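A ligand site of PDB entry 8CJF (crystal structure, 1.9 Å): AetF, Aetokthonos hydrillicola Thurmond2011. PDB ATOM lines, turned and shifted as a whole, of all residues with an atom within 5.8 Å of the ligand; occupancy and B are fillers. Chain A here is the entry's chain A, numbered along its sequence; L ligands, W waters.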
ATOM      1  N   LEU A 191     -19.068 -21.093  21.172  1.00  0.00           N
ATOM      2  CA  LEU A 191     -19.827 -20.192  22.037  1.00  0.00           C
ATOM      3  C   LEU A 191     -21.295 -20.220  21.653  1.00  0.00           C
ATOM      4  O   LEU A 191     -21.639 -20.039  20.482  1.00  0.00           O
ATOM      5  CB  LEU A 191     -19.286 -18.761  21.945  1.00  0.00           C
ATOM      6  CG  LEU A 191     -17.844 -18.548  22.428  1.00  0.00           C
ATOM      7  CD1 LEU A 191     -17.354 -17.153  22.030  1.00  0.00           C
ATOM      8  CD2 LEU A 191     -17.731 -18.755  23.934  1.00  0.00           C
ATOM      9  N   VAL A 195     -27.892 -16.374  24.474  1.00  0.00           N
ATOM     10  CA  VAL A 195     -27.804 -16.679  25.897  1.00  0.00           C
ATOM     11  C   VAL A 195     -28.998 -16.088  26.627  1.00  0.00           C
ATOM     12  O   VAL A 195     -29.690 -15.193  26.131  1.00  0.00           O
ATOM     13  CB  VAL A 195     -26.486 -16.152  26.513  1.00  0.00           C
ATOM     14  CG1 VAL A 195     -25.297 -16.536  25.642  1.00  0.00           C
ATOM     15  CG2 VAL A 195     -26.551 -14.661  26.697  1.00  0.00           C
ATOM     16  N   LEU A 204     -25.178 -13.188  21.538  1.00  0.00           N
ATOM     17  CA  LEU A 204     -23.937 -12.988  22.301  1.00  0.00           C
ATOM     18  C   LEU A 204     -23.295 -11.645  21.990  1.00  0.00           C
ATOM     19  O   LEU A 204     -22.675 -11.037  22.865  1.00  0.00           O
ATOM     20  CB  LEU A 204     -22.956 -14.130  22.017  1.00  0.00           C
ATOM     21  CG  LEU A 204     -22.110 -14.072  20.739  1.00  0.00           C
ATOM     22  CD1 LEU A 204     -20.955 -15.067  20.848  1.00  0.00           C
ATOM     23  CD2 LEU A 204     -22.950 -14.346  19.487  1.00  0.00           C
ATOM     24  N   ASP A 205     -23.415 -11.173  20.742  1.00  0.00           N
ATOM     25  CA  ASP A 205     -22.859  -9.876  20.357  1.00  0.00           C
ATOM     26  C   ASP A 205     -23.431  -8.727  21.167  1.00  0.00           C
ATOM     27  O   ASP A 205     -22.824  -7.648  21.196  1.00  0.00           O
ATOM     28  CB  ASP A 205     -23.128  -9.615  18.873  1.00  0.00           C
ATOM     29  CG  ASP A 205     -24.596  -9.771  18.515  1.00  0.00           C
ATOM     30  OD1 ASP A 205     -25.090 -10.917  18.518  1.00  0.00           O
ATOM     31  OD2 ASP A 205     -25.247  -8.747  18.237  1.00  0.00           O
ATOM     32  N   LEU A 207     -23.769  -8.535  24.391  1.00  0.00           N
ATOM     33  CA  LEU A 207     -23.315  -8.529  25.778  1.00  0.00           C
ATOM     34  C   LEU A 207     -21.819  -8.265  25.913  1.00  0.00           C
ATOM     35  O   LEU A 207     -21.226  -8.599  26.936  1.00  0.00           O
ATOM     36  CB  LEU A 207     -23.674  -9.865  26.433  1.00  0.00           C
ATOM     37  CG  LEU A 207     -25.156 -10.253  26.335  1.00  0.00           C
ATOM     38  CD1 LEU A 207     -25.404 -11.631  26.943  1.00  0.00           C
ATOM     39  CD2 LEU A 207     -26.021  -9.199  26.997  1.00  0.00           C
ATOM     40  N   GLU A 208     -21.207  -7.639  24.908  1.00  0.00           N
ATOM     41  CA  GLU A 208     -19.758  -7.468  24.886  1.00  0.00           C
ATOM     42  C   GLU A 208     -19.300  -6.132  25.437  1.00  0.00           C
ATOM     43  O   GLU A 208     -18.132  -6.018  25.833  1.00  0.00           O
ATOM     44  CB  GLU A 208     -19.231  -7.684  23.458  1.00  0.00           C
ATOM     45  CG  GLU A 208     -19.718  -9.015  22.865  1.00  0.00           C
ATOM     46  CD  GLU A 208     -18.995  -9.432  21.591  1.00  0.00           C
ATOM     47  OE1 GLU A 208     -17.928  -8.855  21.271  1.00  0.00           O
ATOM     48  OE2 GLU A 208     -19.493 -10.356  20.920  1.00  0.00           O
ATOM     49  N   LEU A 223     -13.845  -9.705  32.312  1.00  0.00           N
ATOM     50  CA  LEU A 223     -15.251  -9.769  31.991  1.00  0.00           C
ATOM     51  C   LEU A 223     -15.552 -10.686  30.819  1.00  0.00           C
ATOM     52  O   LEU A 223     -16.674 -11.177  30.708  1.00  0.00           O
ATOM     53  CB  LEU A 223     -15.759  -8.354  31.696  1.00  0.00           C
ATOM     54  CG  LEU A 223     -17.234  -8.182  31.376  1.00  0.00           C
ATOM     55  CD1 LEU A 223     -18.073  -8.641  32.559  1.00  0.00           C
ATOM     56  CD2 LEU A 223     -17.501  -6.720  31.051  1.00  0.00           C
ATOM     57  N   MET A 224     -14.583 -10.926  29.938  1.00  0.00           N
ATOM     58  CA  MET A 224     -14.841 -11.547  28.650  1.00  0.00           C
ATOM     59  C   MET A 224     -14.214 -12.918  28.434  1.00  0.00           C
ATOM     60  O   MET A 224     -14.766 -13.704  27.667  1.00  0.00           O
ATOM     61  CB  MET A 224     -14.347 -10.635  27.513  1.00  0.00           C
ATOM     62  CG  MET A 224     -15.126  -9.346  27.400  1.00  0.00           C
ATOM     63  SD  MET A 224     -16.790  -9.626  26.769  1.00  0.00           S
ATOM     64  CE  MET A 224     -16.448 -10.169  25.085  1.00  0.00           C
ATOM     65  N   MET A 225     -13.085 -13.222  29.070  1.00  0.00           N
ATOM     66  CA  MET A 225     -12.258 -14.323  28.591  1.00  0.00           C
ATOM     67  C   MET A 225     -12.391 -15.614  29.383  1.00  0.00           C
ATOM     68  O   MET A 225     -11.849 -16.639  28.946  1.00  0.00           O
ATOM     69  CB  MET A 225     -10.783 -13.891  28.599  1.00  0.00           C
ATOM     70  CG  MET A 225     -10.486 -12.736  27.657  1.00  0.00           C
ATOM     71  SD  MET A 225     -11.132 -12.978  25.993  1.00  0.00           S
ATOM     72  CE  MET A 225     -10.114 -14.358  25.446  1.00  0.00           C
ATOM     73  N   PRO A 227     -14.876 -17.638  29.434  1.00  0.00           N
ATOM     74  CA  PRO A 227     -15.470 -18.718  28.615  1.00  0.00           C
ATOM     75  C   PRO A 227     -14.505 -19.299  27.599  1.00  0.00           C
ATOM     76  O   PRO A 227     -14.775 -20.374  27.055  1.00  0.00           O
ATOM     77  CB  PRO A 227     -16.655 -18.030  27.914  1.00  0.00           C
ATOM     78  CG  PRO A 227     -16.827 -16.712  28.615  1.00  0.00           C
ATOM     79  CD  PRO A 227     -15.484 -16.341  29.128  1.00  0.00           C
ATOM     80  N   VAL A 228     -13.406 -18.613  27.314  1.00  0.00           N
ATOM     81  CA  VAL A 228     -12.447 -19.040  26.294  1.00  0.00           C
ATOM     82  C   VAL A 228     -11.226 -19.698  26.910  1.00  0.00           C
ATOM     83  O   VAL A 228     -10.821 -20.779  26.493  1.00  0.00           O
ATOM     84  CB  VAL A 228     -12.042 -17.823  25.412  1.00  0.00           C
ATOM     85  CG1 VAL A 228     -10.882 -18.188  24.493  1.00  0.00           C
ATOM     86  CG2 VAL A 228     -13.244 -17.319  24.613  1.00  0.00           C
ATOM     87  N   PRO A 258     -10.766  -9.458  23.830  1.00  0.00           N
ATOM     88  CA  PRO A 258     -10.322 -10.689  23.155  1.00  0.00           C
ATOM     89  C   PRO A 258      -9.250 -10.368  22.115  1.00  0.00           C
ATOM     90  O   PRO A 258      -9.314  -9.340  21.449  1.00  0.00           O
ATOM     91  CB  PRO A 258     -11.611 -11.213  22.498  1.00  0.00           C
ATOM     92  CG  PRO A 258     -12.739 -10.509  23.190  1.00  0.00           C
ATOM     93  CD  PRO A 258     -12.185  -9.169  23.568  1.00  0.00           C
ATOM     94  N   LEU A 262      -8.208 -14.443  17.408  1.00  0.00           N
ATOM     95  CA  LEU A 262      -9.027 -15.479  18.022  1.00  0.00           C
ATOM     96  C   LEU A 262     -10.261 -15.742  17.156  1.00  0.00           C
ATOM     97  O   LEU A 262     -10.882 -14.805  16.655  1.00  0.00           O
ATOM     98  CB  LEU A 262      -9.449 -15.055  19.421  1.00  0.00           C
ATOM     99  CG  LEU A 262     -10.304 -16.034  20.226  1.00  0.00           C
ATOM    100  CD1 LEU A 262      -9.486 -17.260  20.586  1.00  0.00           C
ATOM    101  CD2 LEU A 262     -10.874 -15.362  21.458  1.00  0.00           C
ATOM    102  N   PHE A 380     -14.850 -11.282  15.029  1.00  0.00           N
ATOM    103  CA  PHE A 380     -14.808 -12.379  15.990  1.00  0.00           C
ATOM    104  C   PHE A 380     -16.219 -12.868  16.323  1.00  0.00           C
ATOM    105  O   PHE A 380     -16.459 -14.073  16.404  1.00  0.00           O
ATOM    106  CB  PHE A 380     -14.080 -11.936  17.264  1.00  0.00           C
ATOM    107  CG  PHE A 380     -14.113 -12.943  18.382  1.00  0.00           C
ATOM    108  CD1 PHE A 380     -13.697 -14.253  18.163  1.00  0.00           C
ATOM    109  CD2 PHE A 380     -14.503 -12.582  19.659  1.00  0.00           C
ATOM    110  CE1 PHE A 380     -13.717 -15.178  19.189  1.00  0.00           C
ATOM    111  CE2 PHE A 380     -14.516 -13.500  20.684  1.00  0.00           C
ATOM    112  CZ  PHE A 380     -14.128 -14.799  20.454  1.00  0.00           C
ATOM    113  N   THR A 381     -17.150 -11.938  16.502  1.00  0.00           N
ATOM    114  CA  THR A 381     -18.544 -12.249  16.734  1.00  0.00           C
ATOM    115  C   THR A 381     -19.378 -11.289  15.889  1.00  0.00           C
ATOM    116  O   THR A 381     -18.900 -10.247  15.449  1.00  0.00           O
ATOM    117  CB  THR A 381     -18.946 -12.108  18.211  1.00  0.00           C
ATOM    118  OG1 THR A 381     -18.850 -10.737  18.606  1.00  0.00           O
ATOM    119  CG2 THR A 381     -18.033 -12.935  19.100  1.00  0.00           C
ATOM    120  N   GLN A 508     -22.861  -5.973  34.620  1.00  0.00           N
ATOM    121  CA  GLN A 508     -21.824  -7.003  34.676  1.00  0.00           C
ATOM    122  C   GLN A 508     -20.456  -6.392  34.950  1.00  0.00           C
ATOM    123  O   GLN A 508     -19.749  -6.795  35.882  1.00  0.00           O
ATOM    124  CB  GLN A 508     -21.790  -7.804  33.373  1.00  0.00           C
ATOM    125  CG  GLN A 508     -22.784  -8.948  33.274  1.00  0.00           C
ATOM    126  CD  GLN A 508     -22.435  -9.896  32.136  1.00  0.00           C
ATOM    127  OE1 GLN A 508     -21.495 -10.680  32.228  1.00  0.00           O
ATOM    128  NE2 GLN A 508     -23.201  -9.819  31.062  1.00  0.00           N
ATOM    129  N   TRP A 523     -17.377 -16.000  39.223  1.00  0.00           N
ATOM    130  CA  TRP A 523     -18.619 -15.243  39.217  1.00  0.00           C
ATOM    131  C   TRP A 523     -19.374 -15.428  37.909  1.00  0.00           C
ATOM    132  O   TRP A 523     -20.596 -15.595  37.907  1.00  0.00           O
ATOM    133  CB  TRP A 523     -18.324 -13.760  39.478  1.00  0.00           C
ATOM    134  CG  TRP A 523     -19.543 -12.879  39.476  1.00  0.00           C
ATOM    135  CD1 TRP A 523     -20.319 -12.546  40.543  1.00  0.00           C
ATOM    136  CD2 TRP A 523     -20.106 -12.188  38.350  1.00  0.00           C
ATOM    137  NE1 TRP A 523     -21.337 -11.707  40.153  1.00  0.00           N
ATOM    138  CE2 TRP A 523     -21.222 -11.465  38.811  1.00  0.00           C
ATOM    139  CE3 TRP A 523     -19.771 -12.108  36.993  1.00  0.00           C
ATOM    140  CZ2 TRP A 523     -22.012 -10.685  37.968  1.00  0.00           C
ATOM    141  CZ3 TRP A 523     -20.547 -11.327  36.153  1.00  0.00           C
ATOM    142  CH2 TRP A 523     -21.661 -10.628  36.647  1.00  0.00           C
ATOM    143  N   ASP A 524     -18.655 -15.390  36.782  1.00  0.00           N
ATOM    144  CA  ASP A 524     -19.321 -15.548  35.490  1.00  0.00           C
ATOM    145  C   ASP A 524     -19.974 -16.916  35.350  1.00  0.00           C
ATOM    146  O   ASP A 524     -20.911 -17.063  34.558  1.00  0.00           O
ATOM    147  CB  ASP A 524     -18.306 -15.325  34.349  1.00  0.00           C
ATOM    148  CG  ASP A 524     -18.838 -14.424  33.245  1.00  0.00           C
ATOM    149  OD1 ASP A 524     -19.840 -13.702  33.472  1.00  0.00           O
ATOM    150  OD2 ASP A 524     -18.266 -14.431  32.143  1.00  0.00           O
ATOM    151  N   SER A 531     -23.484 -18.146  30.476  1.00  0.00           N
ATOM    152  CA  SER A 531     -23.711 -17.823  29.061  1.00  0.00           C
ATOM    153  C   SER A 531     -23.314 -18.974  28.149  1.00  0.00           C
ATOM    154  O   SER A 531     -24.059 -19.328  27.222  1.00  0.00           O
ATOM    155  CB  SER A 531     -22.945 -16.557  28.677  1.00  0.00           C
ATOM    156  OG  SER A 531     -23.466 -15.415  29.322  1.00  0.00           O
ATOM    157  N   PHE A 532     -22.140 -19.562  28.366  1.00  0.00           N
ATOM    158  CA  PHE A 532     -21.521 -20.398  27.342  1.00  0.00           C
ATOM    159  C   PHE A 532     -21.186 -21.780  27.867  1.00  0.00           C
ATOM    160  O   PHE A 532     -20.516 -21.927  28.898  1.00  0.00           O
ATOM    161  CB  PHE A 532     -20.270 -19.714  26.809  1.00  0.00           C
ATOM    162  CG  PHE A 532     -20.496 -18.300  26.347  1.00  0.00           C
ATOM    163  CD1 PHE A 532     -21.283 -18.051  25.223  1.00  0.00           C
ATOM    164  CD2 PHE A 532     -19.941 -17.226  27.027  1.00  0.00           C
ATOM    165  CE1 PHE A 532     -21.502 -16.753  24.794  1.00  0.00           C
ATOM    166  CE2 PHE A 532     -20.161 -15.929  26.598  1.00  0.00           C
ATOM    167  CZ  PHE A 532     -20.948 -15.693  25.480  1.00  0.00           C
ATOM    168  N   LYS A 595     -24.039 -14.486  40.285  1.00  0.00           N
ATOM    169  CA  LYS A 595     -24.202 -13.642  39.102  1.00  0.00           C
ATOM    170  C   LYS A 595     -25.660 -13.250  38.908  1.00  0.00           C
ATOM    171  O   LYS A 595     -25.960 -12.088  38.603  1.00  0.00           O
ATOM    172  CB  LYS A 595     -23.665 -14.343  37.854  1.00  0.00           C
ATOM    173  CG  LYS A 595     -23.978 -13.573  36.564  1.00  0.00           C
ATOM    174  CD  LYS A 595     -23.048 -13.943  35.410  1.00  0.00           C
ATOM    175  CE  LYS A 595     -23.322 -13.065  34.190  1.00  0.00           C
ATOM    176  NZ  LYS A 595     -22.671 -13.563  32.938  1.00  0.00           N
HETATM  177  O1  LIG L   1     -21.347 -13.890  29.751  1.00  0.00           O
HETATM  178  C1  LIG L   1     -21.317 -12.646  29.465  1.00  0.00           C
HETATM  179  O2  LIG L   1     -22.436 -12.023  29.209  1.00  0.00           O
HETATM  180  C2  LIG L   1     -19.965 -11.886  29.432  1.00  0.00           C
HETATM  181  N1  LIG L   1     -19.356 -11.949  30.781  1.00  0.00           N
HETATM  182  C3  LIG L   1     -19.037 -12.530  28.359  1.00  0.00           C
HETATM  183  C4  LIG L   1     -19.457 -12.398  26.904  1.00  0.00           C
HETATM  184  C5  LIG L   1     -18.707 -12.793  25.715  1.00  0.00           C
HETATM  185  C6  LIG L   1     -17.426 -13.351  25.614  1.00  0.00           C
HETATM  186  C7  LIG L   1     -16.944 -13.632  24.330  1.00  0.00           C
HETATM  187 BR1  LIG L   1     -15.163 -14.427  24.226  1.00  0.00          BR
HETATM  188  C8  LIG L   1     -17.656 -13.360  23.143  1.00  0.00           C
HETATM  189  C9  LIG L   1     -18.938 -12.785  23.247  1.00  0.00           C
HETATM  190  C10 LIG L   1     -19.468 -12.506  24.557  1.00  0.00           C
HETATM  191  N2  LIG L   1     -20.650 -11.955  24.994  1.00  0.00           N
HETATM  192  C11 LIG L   1     -20.682 -11.888  26.389  1.00  0.00           C
HETATM  193  O   HOH W   1     -19.775 -15.776  30.444  1.00  0.00           O
HETATM  194  O   HOH W   2     -24.492 -12.666  30.883  1.00  0.00           O
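A nitrogen (N1) of the ligand is in salt-bridge range of the side-chain carboxylate (OD2) of Asp 524. The side-chain amino group (NZ) of Lys 595 lies within salt-bridge range of an oxygen (O1) of the ligand (3.5 Å). O of Leu 223 sits at hydrogen-bond distance from N1 of the ligand (2.8 Å). The side-chain hydroxyl (OG) of Ser 531 lies within hydrogen-bond range of an oxygen (O1) of the ligand, at 2.6 Å. The backbone carbonyl oxygen (O) of Leu 204 lies within hydrogen-bond range of a nitrogen (N2) of the ligand, at 3.1 Å. OE1 of Gln 508 sits at hydrogen-bond distance from N1 of the ligand (2.9 Å).
The side-chain amino group (NZ) of Lys 595 lies within salt-bridge range of the side-chain carboxylate (OD1) of Asp 524, 2.9 Å away. The side-chain amino group of Lys 595 is in hydrogen-bond range of the side-chain amide oxygen of Gln 508 (3.2 Å). The side-chain hydroxyl of Thr 381 sits at hydrogen-bond distance from the side-chain carboxylate of Glu 208, at 2.4 Å.
CD1 of Leu 191 touches C8 of the ligand, at 3.96 Å. Leu 207 touches the ligand (O to C11, 3.4 Å). OE2 of Glu 208 touches C9 of the ligand, 3.4 Å away. Met 224 touches the ligand. Val 228 touches the ligand (CG2 to BR1, 3.5 Å). Phe 380 touches the ligand. Phe 532 touches the ligand. Hydrophobic or aromatic side chains that line the ligand: Leu 191, Leu 204, Leu 207, Leu 223, Met 224, Val 228, Phe 380 and Phe 532.
Water W1 lies within hydrogen-bond range of O1 of the ligand (2.6 Å) and OD2 of Asp 524 (2.6 Å). Water W2 lies within hydrogen-bond range of O2 of the ligand (2.7 Å), NZ of Lys 595 (2.9 Å), NE2 of Gln 508 (3.1 Å) and OG of Ser 531 (3.3 Å).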
